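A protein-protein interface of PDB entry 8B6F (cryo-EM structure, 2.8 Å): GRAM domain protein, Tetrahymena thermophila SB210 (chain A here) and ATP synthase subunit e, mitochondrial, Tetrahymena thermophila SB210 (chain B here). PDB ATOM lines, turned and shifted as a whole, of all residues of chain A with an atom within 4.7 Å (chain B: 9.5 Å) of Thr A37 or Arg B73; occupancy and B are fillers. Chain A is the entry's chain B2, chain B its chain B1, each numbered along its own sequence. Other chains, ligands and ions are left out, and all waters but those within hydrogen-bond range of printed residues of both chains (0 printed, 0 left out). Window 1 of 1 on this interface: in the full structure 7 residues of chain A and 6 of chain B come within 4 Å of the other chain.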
ATOM      1  N   ILE A  33       8.372  16.780  -6.435  1.00  0.00           N
ATOM      2  CA  ILE A  33       7.168  17.429  -5.924  1.00  0.00           C
ATOM      3  C   ILE A  33       6.316  16.442  -5.141  1.00  0.00           C
ATOM      4  O   ILE A  33       5.790  16.766  -4.070  1.00  0.00           O
ATOM      5  CB  ILE A  33       6.375  18.073  -7.077  1.00  0.00           C
ATOM      6  CG1 ILE A  33       7.184  19.202  -7.722  1.00  0.00           C
ATOM      7  CG2 ILE A  33       5.026  18.598  -6.586  1.00  0.00           C
ATOM      8  CD1 ILE A  33       7.618  20.291  -6.765  1.00  0.00           C
ATOM      9  N   LYS A  34       6.161  15.226  -5.660  1.00  0.00           N
ATOM     10  CA  LYS A  34       5.308  14.237  -5.018  1.00  0.00           C
ATOM     11  C   LYS A  34       6.056  13.355  -4.032  1.00  0.00           C
ATOM     12  O   LYS A  34       5.442  12.839  -3.090  1.00  0.00           O
ATOM     13  CB  LYS A  34       4.632  13.360  -6.075  1.00  0.00           C
ATOM     14  CG  LYS A  34       3.643  14.115  -6.945  1.00  0.00           C
ATOM     15  CD  LYS A  34       2.736  13.162  -7.701  1.00  0.00           C
ATOM     16  CE  LYS A  34       1.706  13.911  -8.530  1.00  0.00           C
ATOM     17  NZ  LYS A  34       0.825  14.776  -7.700  1.00  0.00           N
ATOM     18  N   MET A  35       7.361  13.170  -4.214  1.00  0.00           N
ATOM     19  CA  MET A  35       8.130  12.251  -3.390  1.00  0.00           C
ATOM     20  C   MET A  35       8.900  12.932  -2.267  1.00  0.00           C
ATOM     21  O   MET A  35       9.610  12.246  -1.524  1.00  0.00           O
ATOM     22  CB  MET A  35       9.108  11.455  -4.259  1.00  0.00           C
ATOM     23  CG  MET A  35       8.441  10.524  -5.252  1.00  0.00           C
ATOM     24  SD  MET A  35       7.189   9.476  -4.488  1.00  0.00           S
ATOM     25  CE  MET A  35       8.065   8.890  -3.039  1.00  0.00           C
ATOM     26  N   CYS A  36       8.784  14.249  -2.120  1.00  0.00           N
ATOM     27  CA  CYS A  36       9.419  14.967  -1.022  1.00  0.00           C
ATOM     28  C   CYS A  36       8.387  15.707  -0.180  1.00  0.00           C
ATOM     29  O   CYS A  36       8.693  16.727   0.440  1.00  0.00           O
ATOM     30  CB  CYS A  36      10.482  15.930  -1.544  1.00  0.00           C
ATOM     31  SG  CYS A  36      11.802  15.103  -2.449  1.00  0.00           S
ATOM     32  N   THR A  37       7.154  15.201  -0.158  1.00  0.00           N
ATOM     33  CA  THR A  37       6.094  15.866   0.590  1.00  0.00           C
ATOM     34  C   THR A  37       6.424  15.931   2.076  1.00  0.00           C
ATOM     35  O   THR A  37       6.208  16.963   2.722  1.00  0.00           O
ATOM     36  CB  THR A  37       4.767  15.142   0.367  1.00  0.00           C
ATOM     37  OG1 THR A  37       4.909  13.758   0.708  1.00  0.00           O
ATOM     38  CG2 THR A  37       4.334  15.259  -1.083  1.00  0.00           C
ATOM     39  N   ALA A  38       6.944  14.840   2.639  1.00  0.00           N
ATOM     40  CA  ALA A  38       7.230  14.814   4.069  1.00  0.00           C
ATOM     41  C   ALA A  38       8.275  15.858   4.443  1.00  0.00           C
ATOM     42  O   ALA A  38       8.068  16.659   5.360  1.00  0.00           O
ATOM     43  CB  ALA A  38       7.697  13.418   4.484  1.00  0.00           C
ATOM     44  N   GLN A  39       9.409  15.866   3.738  1.00  0.00           N
ATOM     45  CA  GLN A  39      10.461  16.825   4.057  1.00  0.00           C
ATOM     46  C   GLN A  39       9.995  18.256   3.833  1.00  0.00           C
ATOM     47  O   GLN A  39      10.266  19.140   4.653  1.00  0.00           O
ATOM     48  CB  GLN A  39      11.710  16.538   3.222  1.00  0.00           C
ATOM     49  CG  GLN A  39      12.465  15.288   3.641  1.00  0.00           C
ATOM     50  CD  GLN A  39      11.829  14.012   3.145  1.00  0.00           C
ATOM     51  OE1 GLN A  39      11.025  14.023   2.216  1.00  0.00           O
ATOM     52  NE2 GLN A  39      12.185  12.896   3.769  1.00  0.00           N
ATOM     53  N   THR A  40       9.295  18.505   2.727  1.00  0.00           N
ATOM     54  CA  THR A  40       8.837  19.858   2.435  1.00  0.00           C
ATOM     55  C   THR A  40       7.834  20.337   3.472  1.00  0.00           C
ATOM     56  O   THR A  40       7.864  21.503   3.885  1.00  0.00           O
ATOM     57  CB  THR A  40       8.238  19.939   1.037  1.00  0.00           C
ATOM     58  OG1 THR A  40       9.140  19.361   0.087  1.00  0.00           O
ATOM     59  CG2 THR A  40       8.026  21.392   0.682  1.00  0.00           C
ATOM     60  N   GLU A  41       6.930  19.457   3.904  1.00  0.00           N
ATOM     61  CA  GLU A  41       5.968  19.837   4.930  1.00  0.00           C
ATOM     62  C   GLU A  41       6.664  20.106   6.256  1.00  0.00           C
ATOM     63  O   GLU A  41       6.283  21.027   6.986  1.00  0.00           O
ATOM     64  CB  GLU A  41       4.913  18.743   5.093  1.00  0.00           C
ATOM     65  CG  GLU A  41       3.771  19.136   6.010  1.00  0.00           C
ATOM     66  CD  GLU A  41       2.634  18.138   5.979  1.00  0.00           C
ATOM     67  OE1 GLU A  41       2.763  17.115   5.275  1.00  0.00           O
ATOM     68  OE2 GLU A  41       1.611  18.377   6.653  1.00  0.00           O
ATOM     69  N   HIS B  65      -6.040  15.457   1.105  1.00  0.00           N
ATOM     70  CA  HIS B  65      -4.653  15.636   0.690  1.00  0.00           C
ATOM     71  C   HIS B  65      -3.710  14.919   1.644  1.00  0.00           C
ATOM     72  O   HIS B  65      -2.776  14.232   1.217  1.00  0.00           O
ATOM     73  CB  HIS B  65      -4.311  17.125   0.624  1.00  0.00           C
ATOM     74  CG  HIS B  65      -4.735  17.792  -0.647  1.00  0.00           C
ATOM     75  ND1 HIS B  65      -3.832  18.318  -1.546  1.00  0.00           N
ATOM     76  CD2 HIS B  65      -5.962  18.031  -1.166  1.00  0.00           C
ATOM     77  CE1 HIS B  65      -4.484  18.847  -2.565  1.00  0.00           C
ATOM     78  NE2 HIS B  65      -5.778  18.687  -2.359  1.00  0.00           N
ATOM     79  N   GLU B  66      -3.936  15.074   2.949  1.00  0.00           N
ATOM     80  CA  GLU B  66      -3.062  14.451   3.936  1.00  0.00           C
ATOM     81  C   GLU B  66      -3.061  12.934   3.792  1.00  0.00           C
ATOM     82  O   GLU B  66      -2.000  12.306   3.728  1.00  0.00           O
ATOM     83  CB  GLU B  66      -3.499  14.859   5.343  1.00  0.00           C
ATOM     84  CG  GLU B  66      -2.643  14.276   6.454  1.00  0.00           C
ATOM     85  CD  GLU B  66      -3.137  14.668   7.833  1.00  0.00           C
ATOM     86  OE1 GLU B  66      -4.228  15.268   7.926  1.00  0.00           O
ATOM     87  OE2 GLU B  66      -2.435  14.377   8.824  1.00  0.00           O
ATOM     88  N   LYS B  67      -4.246  12.324   3.747  1.00  0.00           N
ATOM     89  CA  LYS B  67      -4.319  10.869   3.664  1.00  0.00           C
ATOM     90  C   LYS B  67      -3.742  10.360   2.350  1.00  0.00           C
ATOM     91  O   LYS B  67      -3.073   9.322   2.322  1.00  0.00           O
ATOM     92  CB  LYS B  67      -5.763  10.398   3.835  1.00  0.00           C
ATOM     93  CG  LYS B  67      -6.702  10.865   2.742  1.00  0.00           C
ATOM     94  CD  LYS B  67      -8.138  10.430   3.006  1.00  0.00           C
ATOM     95  CE  LYS B  67      -8.302   8.918   2.938  1.00  0.00           C
ATOM     96  NZ  LYS B  67      -7.873   8.357   1.627  1.00  0.00           N
ATOM     97  N   THR B  68      -3.994  11.073   1.249  1.00  0.00           N
ATOM     98  CA  THR B  68      -3.459  10.644  -0.038  1.00  0.00           C
ATOM     99  C   THR B  68      -1.938  10.696  -0.049  1.00  0.00           C
ATOM    100  O   THR B  68      -1.282   9.773  -0.545  1.00  0.00           O
ATOM    101  CB  THR B  68      -4.031  11.514  -1.157  1.00  0.00           C
ATOM    102  OG1 THR B  68      -5.459  11.407  -1.167  1.00  0.00           O
ATOM    103  CG2 THR B  68      -3.487  11.079  -2.511  1.00  0.00           C
ATOM    104  N   ASN B  69      -1.355  11.765   0.497  1.00  0.00           N
ATOM    105  CA  ASN B  69       0.100  11.848   0.565  1.00  0.00           C
ATOM    106  C   ASN B  69       0.667  10.743   1.444  1.00  0.00           C
ATOM    107  O   ASN B  69       1.696  10.144   1.113  1.00  0.00           O
ATOM    108  CB  ASN B  69       0.524  13.219   1.087  1.00  0.00           C
ATOM    109  CG  ASN B  69       0.153  14.341   0.142  1.00  0.00           C
ATOM    110  OD1 ASN B  69       0.214  14.188  -1.077  1.00  0.00           O
ATOM    111  ND2 ASN B  69      -0.242  15.476   0.701  1.00  0.00           N
ATOM    112  N   GLN B  70       0.014  10.463   2.573  1.00  0.00           N
ATOM    113  CA  GLN B  70       0.476   9.382   3.435  1.00  0.00           C
ATOM    114  C   GLN B  70       0.442   8.051   2.698  1.00  0.00           C
ATOM    115  O   GLN B  70       1.393   7.264   2.773  1.00  0.00           O
ATOM    116  CB  GLN B  70      -0.380   9.320   4.701  1.00  0.00           C
ATOM    117  CG  GLN B  70       0.069   8.270   5.704  1.00  0.00           C
ATOM    118  CD  GLN B  70       1.454   8.542   6.254  1.00  0.00           C
ATOM    119  OE1 GLN B  70       1.627   9.368   7.149  1.00  0.00           O
ATOM    120  NE2 GLN B  70       2.450   7.845   5.719  1.00  0.00           N
ATOM    121  N   ALA B  71      -0.646   7.783   1.975  1.00  0.00           N
ATOM    122  CA  ALA B  71      -0.752   6.534   1.232  1.00  0.00           C
ATOM    123  C   ALA B  71       0.321   6.443   0.156  1.00  0.00           C
ATOM    124  O   ALA B  71       0.921   5.382  -0.045  1.00  0.00           O
ATOM    125  CB  ALA B  71      -2.144   6.409   0.614  1.00  0.00           C
ATOM    126  N   ILE B  72       0.568   7.545  -0.555  1.00  0.00           N
ATOM    127  CA  ILE B  72       1.599   7.543  -1.590  1.00  0.00           C
ATOM    128  C   ILE B  72       2.958   7.230  -0.982  1.00  0.00           C
ATOM    129  O   ILE B  72       3.716   6.404  -1.501  1.00  0.00           O
ATOM    130  CB  ILE B  72       1.612   8.892  -2.331  1.00  0.00           C
ATOM    131  CG1 ILE B  72       0.313   9.084  -3.109  1.00  0.00           C
ATOM    132  CG2 ILE B  72       2.801   8.979  -3.279  1.00  0.00           C
ATOM    133  CD1 ILE B  72       0.028  10.523  -3.449  1.00  0.00           C
ATOM    134  N   ARG B  73       3.289   7.888   0.132  1.00  0.00           N
ATOM    135  CA  ARG B  73       4.584   7.651   0.761  1.00  0.00           C
ATOM    136  C   ARG B  73       4.714   6.206   1.219  1.00  0.00           C
ATOM    137  O   ARG B  73       5.754   5.572   1.008  1.00  0.00           O
ATOM    138  CB  ARG B  73       4.779   8.606   1.938  1.00  0.00           C
ATOM    139  CG  ARG B  73       4.992  10.054   1.528  1.00  0.00           C
ATOM    140  CD  ARG B  73       5.497  10.887   2.695  1.00  0.00           C
ATOM    141  NE  ARG B  73       4.543  10.932   3.797  1.00  0.00           N
ATOM    142  CZ  ARG B  73       3.597  11.850   3.941  1.00  0.00           C
ATOM    143  NH1 ARG B  73       3.441  12.827   3.063  1.00  0.00           N
ATOM    144  NH2 ARG B  73       2.787  11.787   4.993  1.00  0.00           N
ATOM    145  N   ASP B  74       3.670   5.664   1.850  1.00  0.00           N
ATOM    146  CA  ASP B  74       3.731   4.283   2.316  1.00  0.00           C
ATOM    147  C   ASP B  74       3.925   3.320   1.154  1.00  0.00           C
ATOM    148  O   ASP B  74       4.768   2.419   1.210  1.00  0.00           O
ATOM    149  CB  ASP B  74       2.461   3.933   3.092  1.00  0.00           C
ATOM    150  CG  ASP B  74       2.361   4.671   4.410  1.00  0.00           C
ATOM    151  OD1 ASP B  74       3.319   5.388   4.765  1.00  0.00           O
ATOM    152  OD2 ASP B  74       1.326   4.531   5.094  1.00  0.00           O
ATOM    153  N   ALA B  75       3.143   3.493   0.086  1.00  0.00           N
ATOM    154  CA  ALA B  75       3.248   2.581  -1.047  1.00  0.00           C
ATOM    155  C   ALA B  75       4.625   2.647  -1.691  1.00  0.00           C
ATOM    156  O   ALA B  75       5.209   1.610  -2.029  1.00  0.00           O
ATOM    157  CB  ALA B  75       2.164   2.905  -2.076  1.00  0.00           C
ATOM    158  N   VAL B  76       5.163   3.853  -1.872  1.00  0.00           N
ATOM    159  CA  VAL B  76       6.461   3.983  -2.526  1.00  0.00           C
ATOM    160  C   VAL B  76       7.568   3.421  -1.644  1.00  0.00           C
ATOM    161  O   VAL B  76       8.510   2.791  -2.136  1.00  0.00           O
ATOM    162  CB  VAL B  76       6.736   5.445  -2.915  1.00  0.00           C
ATOM    163  CG1 VAL B  76       8.142   5.569  -3.477  1.00  0.00           C
ATOM    164  CG2 VAL B  76       5.709   5.933  -3.922  1.00  0.00           C
ATOM    165  N   LEU B  77       7.482   3.646  -0.332  1.00  0.00           N
ATOM    166  CA  LEU B  77       8.474   3.068   0.568  1.00  0.00           C
ATOM    167  C   LEU B  77       8.446   1.548   0.503  1.00  0.00           C
ATOM    168  O   LEU B  77       9.497   0.902   0.440  1.00  0.00           O
ATOM    169  CB  LEU B  77       8.232   3.546   2.000  1.00  0.00           C
ATOM    170  CG  LEU B  77       9.081   4.723   2.487  1.00  0.00           C
ATOM    171  CD1 LEU B  77      10.527   4.293   2.678  1.00  0.00           C
ATOM    172  CD2 LEU B  77       8.995   5.903   1.529  1.00  0.00           C
ATOM    173  N   GLU B  78       7.250   0.958   0.519  1.00  0.00           N
ATOM    174  CA  GLU B  78       7.153  -0.494   0.445  1.00  0.00           C
ATOM    175  C   GLU B  78       7.712  -1.011  -0.874  1.00  0.00           C
ATOM    176  O   GLU B  78       8.463  -1.993  -0.896  1.00  0.00           O
ATOM    177  CB  GLU B  78       5.697  -0.922   0.632  1.00  0.00           C
ATOM    178  CG  GLU B  78       5.442  -2.406   0.425  1.00  0.00           C
ATOM    179  CD  GLU B  78       4.995  -2.733  -0.987  1.00  0.00           C
ATOM    180  OE1 GLU B  78       5.115  -1.861  -1.872  1.00  0.00           O
ATOM    181  OE2 GLU B  78       4.514  -3.863  -1.213  1.00  0.00           O
ATOM    182  N   LYS B  79       7.361  -0.361  -1.986  1.00  0.00           N
ATOM    183  CA  LYS B  79       7.852  -0.801  -3.288  1.00  0.00           C
ATOM    184  C   LYS B  79       9.367  -0.674  -3.384  1.00  0.00           C
ATOM    185  O   LYS B  79      10.038  -1.560  -3.926  1.00  0.00           O
ATOM    186  CB  LYS B  79       7.178  -0.003  -4.405  1.00  0.00           C
ATOM    187  CG  LYS B  79       5.697  -0.305  -4.583  1.00  0.00           C
ATOM    188  CD  LYS B  79       5.469  -1.746  -5.018  1.00  0.00           C
ATOM    189  CE  LYS B  79       4.006  -2.012  -5.320  1.00  0.00           C
ATOM    190  NZ  LYS B  79       3.531  -1.236  -6.495  1.00  0.00           N
ATOM    191  N   ARG B  80       9.926   0.422  -2.868  1.00  0.00           N
ATOM    192  CA  ARG B  80      11.374   0.595  -2.900  1.00  0.00           C
ATOM    193  C   ARG B  80      12.077  -0.444  -2.039  1.00  0.00           C
ATOM    194  O   ARG B  80      13.138  -0.953  -2.416  1.00  0.00           O
ATOM    195  CB  ARG B  80      11.748   2.007  -2.450  1.00  0.00           C
ATOM    196  CG  ARG B  80      11.430   3.074  -3.481  1.00  0.00           C
ATOM    197  CD  ARG B  80      11.805   4.458  -2.990  1.00  0.00           C
ATOM    198  NE  ARG B  80      11.596   5.463  -4.023  1.00  0.00           N
ATOM    199  CZ  ARG B  80      11.772   6.765  -3.852  1.00  0.00           C
ATOM    200  NH1 ARG B  80      12.157   7.263  -2.688  1.00  0.00           N
ATOM    201  NH2 ARG B  80      11.558   7.589  -4.872  1.00  0.00           N
ATOM    202  N   ALA B  81      11.509  -0.771  -0.878  1.00  0.00           N
ATOM    203  CA  ALA B  81      12.100  -1.814  -0.048  1.00  0.00           C
ATOM    204  C   ALA B  81      12.118  -3.146  -0.785  1.00  0.00           C
ATOM    205  O   ALA B  81      13.126  -3.862  -0.775  1.00  0.00           O
ATOM    206  CB  ALA B  81      11.329  -1.934   1.267  1.00  0.00           C
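The guanidinium group of Arg B73 lies within hydrogen-bond range of the side-chain hydroxyl of Thr A37.
OE1 of Gln B70 lies within hydrogen-bond range of NH2 of Arg B73.
Among the printed residues, pairs that only touch across the chains: Met A35 with Val B76 (3.4 Å) and Ala A38 with Arg B73 (3.8 Å).
Printed residues of chain B within 4 Å of Met A35: Val B76 (3.4 Å).
No residue of chain B comes within 4 Å of Cys A36.
Of chain B, only Arg B73 comes within 4 Å of Thr A37.
Glu B66 touches none of the printed residues of chain A.
Of chain A, only Thr A37 (2.9 Å) and Ala A38 (3.8 Å) come within 4 Å of Arg B73.
Printed residues of chain A within 4 Å of Val B76: Met A35 (3.4 Å).
The nearest printed residue of chain A that does not touch Arg B73 is Glu A41 (4.9 Å).
Printed residues of chain A that touch a printed residue of chain B: Met A35, Thr A37 and Ala A38.
Hydrophobic or aromatic side chains of chain A within 4 Å of the printed part of chain B: Met A35 and Ala A38.
Of the 17 printed residues of chain B, 2 touch a printed residue of chain A.
Printed residues of chain B that touch a printed residue of chain A: Arg B73 and Val B76.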
